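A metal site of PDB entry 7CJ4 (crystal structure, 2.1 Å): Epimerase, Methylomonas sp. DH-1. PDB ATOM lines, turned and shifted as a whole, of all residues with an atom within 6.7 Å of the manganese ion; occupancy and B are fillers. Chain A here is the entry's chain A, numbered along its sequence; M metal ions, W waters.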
ATOM      1  N   HIS A  12     -34.190 -24.398  -5.376  1.00  0.00           N
ATOM      2  CA  HIS A  12     -32.976 -24.691  -6.175  1.00  0.00           C
ATOM      3  C   HIS A  12     -32.631 -26.175  -5.986  1.00  0.00           C
ATOM      4  O   HIS A  12     -32.730 -26.649  -4.840  1.00  0.00           O
ATOM      5  CB  HIS A  12     -31.837 -23.752  -5.805  1.00  0.00           C
ATOM      6  CG  HIS A  12     -30.701 -23.793  -6.770  1.00  0.00           C
ATOM      7  ND1 HIS A  12     -29.653 -24.681  -6.644  1.00  0.00           N
ATOM      8  CD2 HIS A  12     -30.462 -23.067  -7.892  1.00  0.00           C
ATOM      9  CE1 HIS A  12     -28.810 -24.505  -7.635  1.00  0.00           C
ATOM     10  NE2 HIS A  12     -29.279 -23.519  -8.412  1.00  0.00           N
ATOM     11  N   GLU A  41     -36.021 -25.414  -9.614  1.00  0.00           N
ATOM     12  CA  GLU A  41     -35.039 -24.737 -10.488  1.00  0.00           C
ATOM     13  C   GLU A  41     -33.848 -25.686 -10.703  1.00  0.00           C
ATOM     14  O   GLU A  41     -33.092 -25.913  -9.745  1.00  0.00           O
ATOM     15  CB  GLU A  41     -34.607 -23.387  -9.910  1.00  0.00           C
ATOM     16  CG  GLU A  41     -33.708 -22.591 -10.850  1.00  0.00           C
ATOM     17  CD  GLU A  41     -33.199 -21.304 -10.234  1.00  0.00           C
ATOM     18  OE1 GLU A  41     -34.028 -20.460  -9.878  1.00  0.00           O
ATOM     19  OE2 GLU A  41     -31.966 -21.167 -10.083  1.00  0.00           O
ATOM     20  N   GLY A 110     -29.952 -17.074 -13.954  1.00  0.00           N
ATOM     21  CA  GLY A 110     -28.617 -17.287 -13.364  1.00  0.00           C
ATOM     22  C   GLY A 110     -27.538 -16.508 -14.100  1.00  0.00           C
ATOM     23  O   GLY A 110     -27.875 -15.524 -14.784  1.00  0.00           O
ATOM     24  N   GLU A 152     -28.873 -12.825 -13.884  1.00  0.00           N
ATOM     25  CA  GLU A 152     -28.708 -12.747 -12.409  1.00  0.00           C
ATOM     26  C   GLU A 152     -27.523 -11.836 -12.067  1.00  0.00           C
ATOM     27  O   GLU A 152     -26.365 -12.184 -12.427  1.00  0.00           O
ATOM     28  CB  GLU A 152     -28.534 -14.153 -11.820  1.00  0.00           C
ATOM     29  CG  GLU A 152     -28.417 -14.155 -10.301  1.00  0.00           C
ATOM     30  CD  GLU A 152     -28.444 -15.539  -9.675  1.00  0.00           C
ATOM     31  OE1 GLU A 152     -28.152 -16.517 -10.396  1.00  0.00           O
ATOM     32  OE2 GLU A 152     -28.739 -15.636  -8.463  1.00  0.00           O
ATOM     33  N   VAL A 154     -24.804 -10.869  -9.699  1.00  0.00           N
ATOM     34  CA  VAL A 154     -24.063 -11.588  -8.618  1.00  0.00           C
ATOM     35  C   VAL A 154     -22.915 -10.718  -8.107  1.00  0.00           C
ATOM     36  O   VAL A 154     -22.568  -9.722  -8.771  1.00  0.00           O
ATOM     37  CB  VAL A 154     -23.581 -12.978  -9.075  1.00  0.00           C
ATOM     38  CG1 VAL A 154     -24.752 -13.875  -9.429  1.00  0.00           C
ATOM     39  CG2 VAL A 154     -22.587 -12.919 -10.222  1.00  0.00           C
ATOM     40  N   HIS A 183     -32.481 -10.388 -12.975  1.00  0.00           N
ATOM     41  CA  HIS A 183     -32.603 -11.468 -11.965  1.00  0.00           C
ATOM     42  C   HIS A 183     -31.828 -11.030 -10.720  1.00  0.00           C
ATOM     43  O   HIS A 183     -30.609 -10.837 -10.823  1.00  0.00           O
ATOM     44  CB  HIS A 183     -32.137 -12.800 -12.566  1.00  0.00           C
ATOM     45  CG  HIS A 183     -32.100 -13.921 -11.586  1.00  0.00           C
ATOM     46  ND1 HIS A 183     -31.655 -15.176 -11.923  1.00  0.00           N
ATOM     47  CD2 HIS A 183     -32.441 -13.975 -10.277  1.00  0.00           C
ATOM     48  CE1 HIS A 183     -31.743 -15.965 -10.878  1.00  0.00           C
ATOM     49  NE2 HIS A 183     -32.223 -15.261  -9.853  1.00  0.00           N
ATOM     50  N   LEU A 184     -32.539 -10.817  -9.605  1.00  0.00           N
ATOM     51  CA  LEU A 184     -31.944 -10.332  -8.331  1.00  0.00           C
ATOM     52  C   LEU A 184     -31.908 -11.481  -7.317  1.00  0.00           C
ATOM     53  O   LEU A 184     -32.835 -12.322  -7.313  1.00  0.00           O
ATOM     54  CB  LEU A 184     -32.766  -9.164  -7.780  1.00  0.00           C
ATOM     55  CG  LEU A 184     -32.579  -7.808  -8.477  1.00  0.00           C
ATOM     56  CD1 LEU A 184     -33.403  -6.729  -7.784  1.00  0.00           C
ATOM     57  CD2 LEU A 184     -31.107  -7.420  -8.530  1.00  0.00           C
ATOM     58  N   ASP A 185     -30.868 -11.500  -6.489  1.00  0.00           N
ATOM     59  CA  ASP A 185     -30.604 -12.564  -5.492  1.00  0.00           C
ATOM     60  C   ASP A 185     -30.205 -11.884  -4.185  1.00  0.00           C
ATOM     61  O   ASP A 185     -29.189 -11.174  -4.182  1.00  0.00           O
ATOM     62  CB  ASP A 185     -29.533 -13.526  -6.020  1.00  0.00           C
ATOM     63  CG  ASP A 185     -29.249 -14.688  -5.085  1.00  0.00           C
ATOM     64  OD1 ASP A 185     -29.428 -14.493  -3.874  1.00  0.00           O
ATOM     65  OD2 ASP A 185     -28.853 -15.770  -5.587  1.00  0.00           O
ATOM     66  N   TYR A 187     -28.802 -12.808  -1.542  1.00  0.00           N
ATOM     67  CA  TYR A 187     -27.450 -13.195  -1.069  1.00  0.00           C
ATOM     68  C   TYR A 187     -26.427 -12.227  -1.682  1.00  0.00           C
ATOM     69  O   TYR A 187     -25.570 -11.706  -0.938  1.00  0.00           O
ATOM     70  CB  TYR A 187     -27.100 -14.648  -1.414  1.00  0.00           C
ATOM     71  CG  TYR A 187     -25.634 -14.987  -1.316  1.00  0.00           C
ATOM     72  CD1 TYR A 187     -24.994 -15.093  -0.089  1.00  0.00           C
ATOM     73  CD2 TYR A 187     -24.874 -15.196  -2.461  1.00  0.00           C
ATOM     74  CE1 TYR A 187     -23.647 -15.393  -0.008  1.00  0.00           C
ATOM     75  CE2 TYR A 187     -23.523 -15.487  -2.384  1.00  0.00           C
ATOM     76  CZ  TYR A 187     -22.908 -15.596  -1.155  1.00  0.00           C
ATOM     77  OH  TYR A 187     -21.570 -15.902  -1.090  1.00  0.00           O
ATOM     78  N   HIS A 188     -26.511 -11.998  -2.998  1.00  0.00           N
ATOM     79  CA  HIS A 188     -25.589 -11.122  -3.774  1.00  0.00           C
ATOM     80  C   HIS A 188     -25.895  -9.652  -3.461  1.00  0.00           C
ATOM     81  O   HIS A 188     -24.952  -8.854  -3.337  1.00  0.00           O
ATOM     82  CB  HIS A 188     -25.652 -11.452  -5.267  1.00  0.00           C
ATOM     83  CG  HIS A 188     -25.207 -12.836  -5.583  1.00  0.00           C
ATOM     84  ND1 HIS A 188     -23.893 -13.235  -5.398  1.00  0.00           N
ATOM     85  CD2 HIS A 188     -25.874 -13.923  -6.044  1.00  0.00           C
ATOM     86  CE1 HIS A 188     -23.783 -14.508  -5.740  1.00  0.00           C
ATOM     87  NE2 HIS A 188     -24.976 -14.946  -6.147  1.00  0.00           N
ATOM     88  N   HIS A 211     -34.098 -14.666  -6.557  1.00  0.00           N
ATOM     89  CA  HIS A 211     -33.493 -15.681  -5.668  1.00  0.00           C
ATOM     90  C   HIS A 211     -33.516 -15.154  -4.230  1.00  0.00           C
ATOM     91  O   HIS A 211     -32.983 -14.055  -3.998  1.00  0.00           O
ATOM     92  CB  HIS A 211     -32.070 -16.035  -6.108  1.00  0.00           C
ATOM     93  CG  HIS A 211     -32.045 -17.064  -7.188  1.00  0.00           C
ATOM     94  ND1 HIS A 211     -30.878 -17.670  -7.608  1.00  0.00           N
ATOM     95  CD2 HIS A 211     -33.052 -17.619  -7.905  1.00  0.00           C
ATOM     96  CE1 HIS A 211     -31.162 -18.538  -8.564  1.00  0.00           C
ATOM     97  NE2 HIS A 211     -32.489 -18.533  -8.746  1.00  0.00           N
ATOM     98  N   ILE A 212     -34.141 -15.925  -3.326  1.00  0.00           N
ATOM     99  CA  ILE A 212     -34.104 -15.702  -1.852  1.00  0.00           C
ATOM    100  C   ILE A 212     -32.966 -16.548  -1.286  1.00  0.00           C
ATOM    101  O   ILE A 212     -33.118 -17.789  -1.279  1.00  0.00           O
ATOM    102  CB  ILE A 212     -35.449 -16.055  -1.196  1.00  0.00           C
ATOM    103  CG1 ILE A 212     -36.619 -15.291  -1.824  1.00  0.00           C
ATOM    104  CG2 ILE A 212     -35.371 -15.842   0.306  1.00  0.00           C
ATOM    105  CD1 ILE A 212     -36.344 -13.834  -2.015  1.00  0.00           C
ATOM    106  N   ARG A 217     -26.076 -18.095   3.082  1.00  0.00           N
ATOM    107  CA  ARG A 217     -26.758 -19.068   2.165  1.00  0.00           C
ATOM    108  C   ARG A 217     -27.248 -20.287   2.943  1.00  0.00           C
ATOM    109  O   ARG A 217     -27.422 -21.362   2.323  1.00  0.00           O
ATOM    110  CB  ARG A 217     -25.825 -19.479   1.026  1.00  0.00           C
ATOM    111  CG  ARG A 217     -25.191 -18.300   0.300  1.00  0.00           C
ATOM    112  CD  ARG A 217     -24.697 -18.667  -1.095  1.00  0.00           C
ATOM    113  NE  ARG A 217     -25.608 -18.231  -2.145  1.00  0.00           N
ATOM    114  CZ  ARG A 217     -25.313 -18.227  -3.445  1.00  0.00           C
ATOM    115  NH1 ARG A 217     -24.131 -18.654  -3.852  1.00  0.00           N
ATOM    116  NH2 ARG A 217     -26.194 -17.799  -4.317  1.00  0.00           N
ATOM    117  N   GLU A 246     -32.717 -20.604  -2.564  1.00  0.00           N
ATOM    118  CA  GLU A 246     -31.370 -21.075  -2.980  1.00  0.00           C
ATOM    119  C   GLU A 246     -30.553 -21.228  -1.696  1.00  0.00           C
ATOM    120  O   GLU A 246     -30.615 -20.330  -0.838  1.00  0.00           O
ATOM    121  CB  GLU A 246     -30.762 -20.064  -3.971  1.00  0.00           C
ATOM    122  CG  GLU A 246     -29.500 -20.542  -4.648  1.00  0.00           C
ATOM    123  CD  GLU A 246     -28.899 -19.584  -5.677  1.00  0.00           C
ATOM    124  OE1 GLU A 246     -28.147 -20.044  -6.548  1.00  0.00           O
ATOM    125  OE2 GLU A 246     -29.174 -18.385  -5.590  1.00  0.00           O
ATOM    126  N   PHE A 248     -26.859 -23.621  -0.029  1.00  0.00           N
ATOM    127  CA  PHE A 248     -25.658 -24.453  -0.280  1.00  0.00           C
ATOM    128  C   PHE A 248     -25.012 -24.818   1.059  1.00  0.00           C
ATOM    129  O   PHE A 248     -24.665 -23.913   1.856  1.00  0.00           O
ATOM    130  CB  PHE A 248     -24.687 -23.732  -1.211  1.00  0.00           C
ATOM    131  CG  PHE A 248     -25.245 -23.432  -2.577  1.00  0.00           C
ATOM    132  CD1 PHE A 248     -25.273 -24.406  -3.561  1.00  0.00           C
ATOM    133  CD2 PHE A 248     -25.782 -22.191  -2.871  1.00  0.00           C
ATOM    134  CE1 PHE A 248     -25.793 -24.140  -4.816  1.00  0.00           C
ATOM    135  CE2 PHE A 248     -26.311 -21.922  -4.123  1.00  0.00           C
ATOM    136  CZ  PHE A 248     -26.320 -22.894  -5.094  1.00  0.00           C
HETATM  137 MN    MN M   1     -28.822 -17.227  -7.113  1.00  0.00          MN
HETATM  138  O   HOH W   1     -26.729 -17.769  -7.454  1.00  0.00           O
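Arg 217 touches the manganese ion (NH2 to MN, 3.9 Å).
Within 4 Å of the manganese ion: Glu 152, Asp 185, His 211, Arg 217 and Glu 246.
The nearest printed residue that does not touch the manganese ion is His 188 (4.6 Å).
Water W1 lies within hydrogen-bond range of the side-chain carboxylate (OE1) of Glu 246 (2.8 Å), the guanidinium group (NH2) of Arg 217 (3.2 Å) and the side-chain carboxylate (OE1) of Glu 152 (3.5 Å).
The side-chain carboxylate (OE1) of Glu 41 is in hydrogen-bond range of a ring nitrogen (NE2) of His 211 (2.7 Å).
N of Glu 246 sits at hydrogen-bond distance from O of Ile 212 (3.1 Å).
The side-chain carboxylate (OE1) of Glu 246 is in salt-bridge range of the guanidinium group (NH2) of Arg 217 (3.7 Å).
N of Glu 152 lies within hydrogen-bond range of O of Gly 110, 3.0 Å away.
The backbone carbonyl oxygen of Arg 217 sits at hydrogen-bond distance from the backbone NH of Phe 248 (3.3 Å).
The backbone NH (N) of His 211 lies within hydrogen-bond range of the backbone carbonyl oxygen (O) of Leu 184, 2.8 Å away.
OD2 of Asp 185 sits close to NH2 of Arg 217 (3.6 Å).
The backbone NH (N) of Tyr 187 is in hydrogen-bond range of the side-chain carboxylate (OD1) of Asp 185.
The manganese ion is bound by the side-chain carboxylate (OE2) of Glu 246 (1.9 Å).
The manganese ion is bound by OE2 of Glu 152, 2.1 Å away.
The side-chain carboxylate (OD2) of Asp 185 is bound to the manganese ion, 2.1 Å away.
The manganese ion is bound by a ring nitrogen (ND1) of His 211 (2.2 Å).
Water W1 is bound to the manganese ion (2.2 Å).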
